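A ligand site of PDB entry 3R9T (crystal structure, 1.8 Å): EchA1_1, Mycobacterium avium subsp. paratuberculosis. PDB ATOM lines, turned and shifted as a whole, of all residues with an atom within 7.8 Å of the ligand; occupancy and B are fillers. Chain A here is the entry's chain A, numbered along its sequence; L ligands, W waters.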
ATOM      1  N   ALA A  69      11.325   1.552  -6.313  1.00  0.00           N
ATOM      2  CA  ALA A  69      11.272   2.203  -7.623  1.00  0.00           C
ATOM      3  C   ALA A  69       9.905   2.731  -7.983  1.00  0.00           C
ATOM      4  O   ALA A  69       9.752   3.398  -9.009  1.00  0.00           O
ATOM      5  CB  ALA A  69      11.732   1.258  -8.709  1.00  0.00           C
ATOM      6  N   GLY A  70       8.915   2.436  -7.153  1.00  0.00           N
ATOM      7  CA  GLY A  70       7.602   2.996  -7.340  1.00  0.00           C
ATOM      8  C   GLY A  70       6.506   1.975  -7.219  1.00  0.00           C
ATOM      9  O   GLY A  70       6.716   0.870  -6.682  1.00  0.00           O
ATOM     10  N   ALA A  71       5.331   2.377  -7.689  1.00  0.00           N
ATOM     11  CA  ALA A  71       4.155   1.523  -7.787  1.00  0.00           C
ATOM     12  C   ALA A  71       4.421   0.446  -8.819  1.00  0.00           C
ATOM     13  O   ALA A  71       4.936   0.748  -9.906  1.00  0.00           O
ATOM     14  CB  ALA A  71       2.947   2.361  -8.226  1.00  0.00           C
ATOM     15  N   ASP A  72       4.094  -0.805  -8.493  1.00  0.00           N
ATOM     16  CA  ASP A  72       4.341  -1.911  -9.425  1.00  0.00           C
ATOM     17  C   ASP A  72       3.539  -1.704 -10.708  1.00  0.00           C
ATOM     18  O   ASP A  72       2.311  -1.683 -10.693  1.00  0.00           O
ATOM     19  CB  ASP A  72       4.027  -3.264  -8.793  1.00  0.00           C
ATOM     20  CG  ASP A  72       4.476  -4.437  -9.664  1.00  0.00           C
ATOM     21  OD1 ASP A  72       3.793  -4.725 -10.671  1.00  0.00           O
ATOM     22  OD2 ASP A  72       5.501  -5.081  -9.325  1.00  0.00           O
ATOM     23  N   LEU A  73       4.241  -1.524 -11.820  1.00  0.00           N
ATOM     24  CA  LEU A  73       3.598  -1.148 -13.077  1.00  0.00           C
ATOM     25  C   LEU A  73       2.790  -2.288 -13.726  1.00  0.00           C
ATOM     26  O   LEU A  73       1.774  -2.031 -14.380  1.00  0.00           O
ATOM     27  CB  LEU A  73       4.621  -0.577 -14.069  1.00  0.00           C
ATOM     28  CG  LEU A  73       5.073   0.864 -13.829  1.00  0.00           C
ATOM     29  CD1 LEU A  73       6.279   1.188 -14.712  1.00  0.00           C
ATOM     30  CD2 LEU A  73       3.939   1.837 -14.105  1.00  0.00           C
ATOM     31  N   ILE A  76      -0.445  -2.266 -11.871  1.00  0.00           N
ATOM     32  CA  ILE A  76      -1.241  -1.140 -12.365  1.00  0.00           C
ATOM     33  C   ILE A  76      -1.890  -1.520 -13.702  1.00  0.00           C
ATOM     34  O   ILE A  76      -3.093  -1.318 -13.888  1.00  0.00           O
ATOM     35  CB  ILE A  76      -0.401   0.129 -12.527  1.00  0.00           C
ATOM     36  CG1 ILE A  76      -0.105   0.727 -11.148  1.00  0.00           C
ATOM     37  CG2 ILE A  76      -1.114   1.156 -13.403  1.00  0.00           C
ATOM     38  CD1 ILE A  76       1.151   1.572 -11.127  1.00  0.00           C
ATOM     39  N   GLU A  80      -4.896  -4.078 -10.602  1.00  0.00           N
ATOM     40  CA  GLU A  80      -4.839  -4.670  -9.260  1.00  0.00           C
ATOM     41  C   GLU A  80      -4.885  -3.533  -8.260  1.00  0.00           C
ATOM     42  O   GLU A  80      -4.354  -2.445  -8.534  1.00  0.00           O
ATOM     43  CB  GLU A  80      -3.532  -5.431  -9.031  1.00  0.00           C
ATOM     44  CG  GLU A  80      -3.445  -6.828  -9.554  1.00  0.00           C
ATOM     45  CD  GLU A  80      -2.038  -7.397  -9.382  1.00  0.00           C
ATOM     46  OE1 GLU A  80      -1.373  -7.156  -8.344  1.00  0.00           O
ATOM     47  OE2 GLU A  80      -1.592  -8.106 -10.314  1.00  0.00           O
ATOM     48  N   LEU A  82      -3.247  -1.926  -5.129  1.00  0.00           N
ATOM     49  CA  LEU A  82      -1.854  -1.940  -4.637  1.00  0.00           C
ATOM     50  C   LEU A  82      -1.808  -1.876  -3.111  1.00  0.00           C
ATOM     51  O   LEU A  82      -0.766  -2.115  -2.523  1.00  0.00           O
ATOM     52  CB  LEU A  82      -1.066  -0.732  -5.167  1.00  0.00           C
ATOM     53  CG  LEU A  82      -1.017  -0.516  -6.684  1.00  0.00           C
ATOM     54  CD1 LEU A  82      -0.150   0.681  -7.063  1.00  0.00           C
ATOM     55  CD2 LEU A  82      -0.554  -1.773  -7.419  1.00  0.00           C
ATOM     56  N   PHE A  92      -1.395   3.662   0.055  1.00  0.00           N
ATOM     57  CA  PHE A  92      -0.284   3.044  -0.649  1.00  0.00           C
ATOM     58  C   PHE A  92       0.768   2.455   0.314  1.00  0.00           C
ATOM     59  O   PHE A  92       1.200   3.106   1.280  1.00  0.00           O
ATOM     60  CB  PHE A  92       0.349   4.122  -1.534  1.00  0.00           C
ATOM     61  CG  PHE A  92       1.449   3.649  -2.420  1.00  0.00           C
ATOM     62  CD1 PHE A  92       1.166   3.017  -3.628  1.00  0.00           C
ATOM     63  CD2 PHE A  92       2.770   3.923  -2.106  1.00  0.00           C
ATOM     64  CE1 PHE A  92       2.178   2.642  -4.477  1.00  0.00           C
ATOM     65  CE2 PHE A  92       3.789   3.541  -2.966  1.00  0.00           C
ATOM     66  CZ  PHE A  92       3.489   2.890  -4.152  1.00  0.00           C
ATOM     67  N   VAL A  96       1.374   5.260   3.586  1.00  0.00           N
ATOM     68  CA  VAL A  96       1.301   6.715   3.361  1.00  0.00           C
ATOM     69  C   VAL A  96       0.139   7.421   4.033  1.00  0.00           C
ATOM     70  O   VAL A  96       0.165   8.636   4.168  1.00  0.00           O
ATOM     71  CB  VAL A  96       1.287   7.087   1.875  1.00  0.00           C
ATOM     72  CG1 VAL A  96       2.555   6.605   1.198  1.00  0.00           C
ATOM     73  CG2 VAL A  96       0.041   6.564   1.172  1.00  0.00           C
ATOM     74  N   LEU A 113      11.975   6.417  -6.313  1.00  0.00           N
ATOM     75  CA  LEU A 113      11.266   7.206  -7.330  1.00  0.00           C
ATOM     76  C   LEU A 113       9.770   6.969  -7.244  1.00  0.00           C
ATOM     77  O   LEU A 113       9.322   5.848  -6.974  1.00  0.00           O
ATOM     78  CB  LEU A 113      11.752   6.874  -8.742  1.00  0.00           C
ATOM     79  CG  LEU A 113      13.232   7.194  -8.995  1.00  0.00           C
ATOM     80  CD1 LEU A 113      13.610   6.650 -10.353  1.00  0.00           C
ATOM     81  CD2 LEU A 113      13.557   8.685  -8.911  1.00  0.00           C
ATOM     82  N   GLY A 114       9.001   8.026  -7.449  1.00  0.00           N
ATOM     83  CA  GLY A 114       7.549   7.933  -7.500  1.00  0.00           C
ATOM     84  C   GLY A 114       7.065   7.499  -6.132  1.00  0.00           C
ATOM     85  O   GLY A 114       7.312   8.196  -5.125  1.00  0.00           O
ATOM     86  N   GLY A 115       6.417   6.337  -6.079  1.00  0.00           N
ATOM     87  CA  GLY A 115       6.003   5.740  -4.806  1.00  0.00           C
ATOM     88  C   GLY A 115       7.084   5.730  -3.747  1.00  0.00           C
ATOM     89  O   GLY A 115       6.781   5.925  -2.557  1.00  0.00           O
ATOM     90  N   GLY A 116       8.330   5.507  -4.146  1.00  0.00           N
ATOM     91  CA  GLY A 116       9.449   5.496  -3.212  1.00  0.00           C
ATOM     92  C   GLY A 116       9.704   6.842  -2.574  1.00  0.00           C
ATOM     93  O   GLY A 116       9.987   6.935  -1.375  1.00  0.00           O
ATOM     94  N   GLU A 118       7.330   9.021  -2.303  1.00  0.00           N
ATOM     95  CA  GLU A 118       6.124   9.169  -1.484  1.00  0.00           C
ATOM     96  C   GLU A 118       6.202   8.443  -0.108  1.00  0.00           C
ATOM     97  O   GLU A 118       5.654   8.926   0.905  1.00  0.00           O
ATOM     98  CB  GLU A 118       4.899   8.763  -2.298  1.00  0.00           C
ATOM     99  CG  GLU A 118       4.675   9.695  -3.526  1.00  0.00           C
ATOM    100  CD  GLU A 118       3.584   9.197  -4.398  1.00  0.00           C
ATOM    101  OE1 GLU A 118       3.803   8.154  -5.055  1.00  0.00           O
ATOM    102  OE2 GLU A 118       2.495   9.810  -4.421  1.00  0.00           O
ATOM    103  N   LEU A 136       9.438  12.353  -8.726  1.00  0.00           N
ATOM    104  CA  LEU A 136       8.039  11.990  -8.970  1.00  0.00           C
ATOM    105  C   LEU A 136       7.830  11.926 -10.486  1.00  0.00           C
ATOM    106  O   LEU A 136       7.254  12.840 -11.098  1.00  0.00           O
ATOM    107  CB  LEU A 136       7.108  13.016  -8.287  1.00  0.00           C
ATOM    108  CG  LEU A 136       7.168  13.137  -6.752  1.00  0.00           C
ATOM    109  CD1 LEU A 136       6.241  14.271  -6.294  1.00  0.00           C
ATOM    110  CD2 LEU A 136       6.788  11.826  -6.058  1.00  0.00           C
ATOM    111  N   PRO A 137       8.268  10.807 -11.115  1.00  0.00           N
ATOM    112  CA  PRO A 137       8.199  10.709 -12.581  1.00  0.00           C
ATOM    113  C   PRO A 137       6.840  10.240 -13.130  1.00  0.00           C
ATOM    114  O   PRO A 137       6.735   9.925 -14.304  1.00  0.00           O
ATOM    115  CB  PRO A 137       9.310   9.692 -12.923  1.00  0.00           C
ATOM    116  CG  PRO A 137       9.374   8.821 -11.730  1.00  0.00           C
ATOM    117  CD  PRO A 137       8.998   9.668 -10.527  1.00  0.00           C
ATOM    118  N   GLU A 138       5.811  10.238 -12.280  1.00  0.00           N
ATOM    119  CA  GLU A 138       4.482   9.744 -12.652  1.00  0.00           C
ATOM    120  C   GLU A 138       3.944  10.495 -13.861  1.00  0.00           C
ATOM    121  O   GLU A 138       3.262   9.913 -14.739  1.00  0.00           O
ATOM    122  CB  GLU A 138       3.492   9.855 -11.483  1.00  0.00           C
ATOM    123  CG  GLU A 138       3.695   8.853 -10.301  1.00  0.00           C
ATOM    124  CD  GLU A 138       4.643   9.350  -9.217  1.00  0.00           C
ATOM    125  OE1 GLU A 138       5.426  10.286  -9.473  1.00  0.00           O
ATOM    126  OE2 GLU A 138       4.617   8.790  -8.087  1.00  0.00           O
ATOM    127  N   VAL A 139       4.241  11.781 -13.924  1.00  0.00           N
ATOM    128  CA  VAL A 139       3.817  12.614 -15.055  1.00  0.00           C
ATOM    129  C   VAL A 139       4.355  12.168 -16.415  1.00  0.00           C
ATOM    130  O   VAL A 139       3.771  12.482 -17.444  1.00  0.00           O
ATOM    131  CB  VAL A 139       4.125  14.101 -14.814  1.00  0.00           C
ATOM    132  CG1 VAL A 139       3.228  14.620 -13.693  1.00  0.00           C
ATOM    133  CG2 VAL A 139       5.636  14.344 -14.580  1.00  0.00           C
ATOM    134  N   LEU A 143       0.316   9.110 -15.377  1.00  0.00           N
ATOM    135  CA  LEU A 143      -0.348   8.976 -14.073  1.00  0.00           C
ATOM    136  C   LEU A 143      -0.015  10.203 -13.212  1.00  0.00           C
ATOM    137  O   LEU A 143       0.438  11.207 -13.743  1.00  0.00           O
ATOM    138  CB  LEU A 143       0.101   7.676 -13.393  1.00  0.00           C
ATOM    139  CG  LEU A 143      -0.267   6.443 -14.245  1.00  0.00           C
ATOM    140  CD1 LEU A 143       0.409   5.159 -13.745  1.00  0.00           C
ATOM    141  CD2 LEU A 143      -1.768   6.282 -14.284  1.00  0.00           C
ATOM    142  N   ILE A 144      -0.240  10.131 -11.897  1.00  0.00           N
ATOM    143  CA  ILE A 144       0.155  11.214 -10.963  1.00  0.00           C
ATOM    144  C   ILE A 144       0.653  10.543  -9.688  1.00  0.00           C
ATOM    145  O   ILE A 144       0.409   9.345  -9.484  1.00  0.00           O
ATOM    146  CB  ILE A 144      -0.975  12.241 -10.642  1.00  0.00           C
ATOM    147  CG1 ILE A 144      -2.244  11.542 -10.107  1.00  0.00           C
ATOM    148  CG2 ILE A 144      -1.339  13.100 -11.870  1.00  0.00           C
ATOM    149  CD1 ILE A 144      -3.279  12.478  -9.458  1.00  0.00           C
ATOM    150  N   ALA A 145       1.334  11.306  -8.823  1.00  0.00           N
ATOM    151  CA  ALA A 145       1.793  10.849  -7.522  1.00  0.00           C
ATOM    152  C   ALA A 145       0.616  10.770  -6.582  1.00  0.00           C
ATOM    153  O   ALA A 145       0.400  11.649  -5.768  1.00  0.00           O
ATOM    154  CB  ALA A 145       2.867  11.801  -6.953  1.00  0.00           C
ATOM    155  N   ALA A 146      -0.150   9.708  -6.727  1.00  0.00           N
ATOM    156  CA  ALA A 146      -1.439   9.597  -6.067  1.00  0.00           C
ATOM    157  C   ALA A 146      -1.314   9.156  -4.610  1.00  0.00           C
ATOM    158  O   ALA A 146      -2.289   9.239  -3.834  1.00  0.00           O
ATOM    159  CB  ALA A 146      -2.324   8.596  -6.839  1.00  0.00           C
ATOM    160  N   ALA A 147      -0.133   8.700  -4.229  1.00  0.00           N
ATOM    161  CA  ALA A 147       0.134   8.270  -2.858  1.00  0.00           C
ATOM    162  C   ALA A 147       0.661   9.414  -1.982  1.00  0.00           C
ATOM    163  O   ALA A 147       1.571   9.225  -1.138  1.00  0.00           O
ATOM    164  CB  ALA A 147       1.138   7.122  -2.882  1.00  0.00           C
ATOM    165  N   GLY A 148       0.047  10.583  -2.160  1.00  0.00           N
ATOM    166  CA  GLY A 148       0.328  11.767  -1.338  1.00  0.00           C
ATOM    167  C   GLY A 148       1.342  12.743  -1.925  1.00  0.00           C
ATOM    168  O   GLY A 148       1.418  13.888  -1.481  1.00  0.00           O
ATOM    169  N   GLY A 149       2.112  12.323  -2.938  1.00  0.00           N
ATOM    170  CA  GLY A 149       3.195  13.151  -3.506  1.00  0.00           C
ATOM    171  C   GLY A 149       2.702  14.487  -4.039  1.00  0.00           C
ATOM    172  O   GLY A 149       3.360  15.515  -3.807  1.00  0.00           O
ATOM    173  N   VAL A 150       1.574  14.503  -4.735  1.00  0.00           N
ATOM    174  CA  VAL A 150       1.134  15.741  -5.361  1.00  0.00           C
ATOM    175  C   VAL A 150       0.885  16.888  -4.368  1.00  0.00           C
ATOM    176  O   VAL A 150       1.226  18.042  -4.662  1.00  0.00           O
ATOM    177  CB  VAL A 150      -0.075  15.589  -6.272  1.00  0.00           C
ATOM    178  CG1 VAL A 150      -0.391  16.940  -6.899  1.00  0.00           C
ATOM    179  CG2 VAL A 150       0.194  14.604  -7.382  1.00  0.00           C
ATOM    180  N   THR A 236      -6.887  14.326  -4.691  1.00  0.00           N
ATOM    181  CA  THR A 236      -6.066  13.321  -5.349  1.00  0.00           C
ATOM    182  C   THR A 236      -6.913  12.152  -5.860  1.00  0.00           C
ATOM    183  O   THR A 236      -6.774  11.716  -7.005  1.00  0.00           O
ATOM    184  CB  THR A 236      -5.012  12.791  -4.408  1.00  0.00           C
ATOM    185  OG1 THR A 236      -4.123  13.868  -4.065  1.00  0.00           O
ATOM    186  CG2 THR A 236      -4.196  11.673  -5.088  1.00  0.00           C
ATOM    187  N   MET A 240      -7.418  11.043  -9.708  1.00  0.00           N
ATOM    188  CA  MET A 240      -6.824   9.783 -10.121  1.00  0.00           C
ATOM    189  C   MET A 240      -7.882   8.932 -10.816  1.00  0.00           C
ATOM    190  O   MET A 240      -7.639   8.373 -11.882  1.00  0.00           O
ATOM    191  CB  MET A 240      -6.240   9.037  -8.912  1.00  0.00           C
ATOM    192  CG  MET A 240      -5.380   7.811  -9.269  1.00  0.00           C
ATOM    193  SD  MET A 240      -4.032   8.186 -10.383  1.00  0.00           S
ATOM    194  CE  MET A 240      -3.013   6.711 -10.161  1.00  0.00           C
ATOM    195  N   LEU A 244      -7.250   7.660 -14.663  1.00  0.00           N
ATOM    196  CA  LEU A 244      -7.070   6.230 -14.965  1.00  0.00           C
ATOM    197  C   LEU A 244      -7.940   5.770 -16.132  1.00  0.00           C
ATOM    198  O   LEU A 244      -7.672   4.735 -16.726  1.00  0.00           O
ATOM    199  CB  LEU A 244      -7.369   5.369 -13.737  1.00  0.00           C
ATOM    200  CG  LEU A 244      -6.281   5.296 -12.655  1.00  0.00           C
ATOM    201  CD1 LEU A 244      -6.751   4.546 -11.435  1.00  0.00           C
ATOM    202  CD2 LEU A 244      -4.963   4.685 -13.154  1.00  0.00           C
HETATM  203  C1  LIG L   1       2.007   6.710  -7.360  1.00  0.00           C
HETATM  204  O1  LIG L   1       1.885   7.349  -6.293  1.00  0.00           O
HETATM  205  O2  LIG L   1       3.022   6.821  -8.085  1.00  0.00           O
HETATM  206  C2  LIG L   1       0.897   5.787  -7.792  1.00  0.00           C
HETATM  207  C3  LIG L   1       0.843   5.374  -9.113  1.00  0.00           C
HETATM  208  C4  LIG L   1      -0.177   4.508  -9.518  1.00  0.00           C
HETATM  209  C5  LIG L   1      -1.131   4.084  -8.604  1.00  0.00           C
HETATM  210  C6  LIG L   1      -1.086   4.501  -7.282  1.00  0.00           C
HETATM  211  C7  LIG L   1      -0.057   5.363  -6.877  1.00  0.00           C
HETATM  212  O   HOH W   1       5.219   5.143  -8.516  1.00  0.00           O
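The side-chain carboxylate (OE1) of Glu 118 sits close to an oxygen (O1) of the ligand (2.4 Å). The backbone NH of Ala 147 sits at hydrogen-bond distance from an oxygen (O1) of the ligand (3.2 Å). The side-chain carboxylate of Glu 138 sits close to an oxygen (O2) of the ligand (2.5 Å). The backbone NH of Ala 146 is in hydrogen-bond range of an oxygen (O1) of the ligand.
Water W1 lies within hydrogen-bond range of an oxygen (O2) of the ligand, the backbone NH of Ala 71 and the backbone NH of Gly 115.
Residues that only touch the ligand: Met 240 (3.6 Å), Ile 76 (3.6 Å), Ala 145 (3.7 Å), Ile 144 (3.7 Å), Ala 71 (3.8 Å), Leu 82 (3.9 Å) and Gly 115 (3.97 Å). Within 4 Å of the ligand: Ala 71, Ile 76, Leu 82, Gly 115, Glu 118, Glu 138, Ile 144, Ala 145, Ala 146, Ala 147 and Met 240. The nearest printed residue that does not touch the ligand is Phe 92 (4.2 Å).
The backbone NH of Leu 143 lies within hydrogen-bond range of the backbone carbonyl oxygen of Glu 138 (3.1 Å). The side-chain carboxylate (OE2) of Glu 118 sits at hydrogen-bond distance from the backbone NH (N) of Gly 149, at 2.9 Å. The side-chain carboxylate (OE2) of Glu 118 is in hydrogen-bond range of the backbone NH (N) of Ala 147 (2.9 Å). The backbone NH of Val 150 sits at hydrogen-bond distance from the backbone carbonyl oxygen of Ala 145 (3.3 Å). OE1 of Glu 118 sits close to N of Gly 115 (3.3 Å). N of Gly 148 lies within hydrogen-bond range of OE2 of Glu 118.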
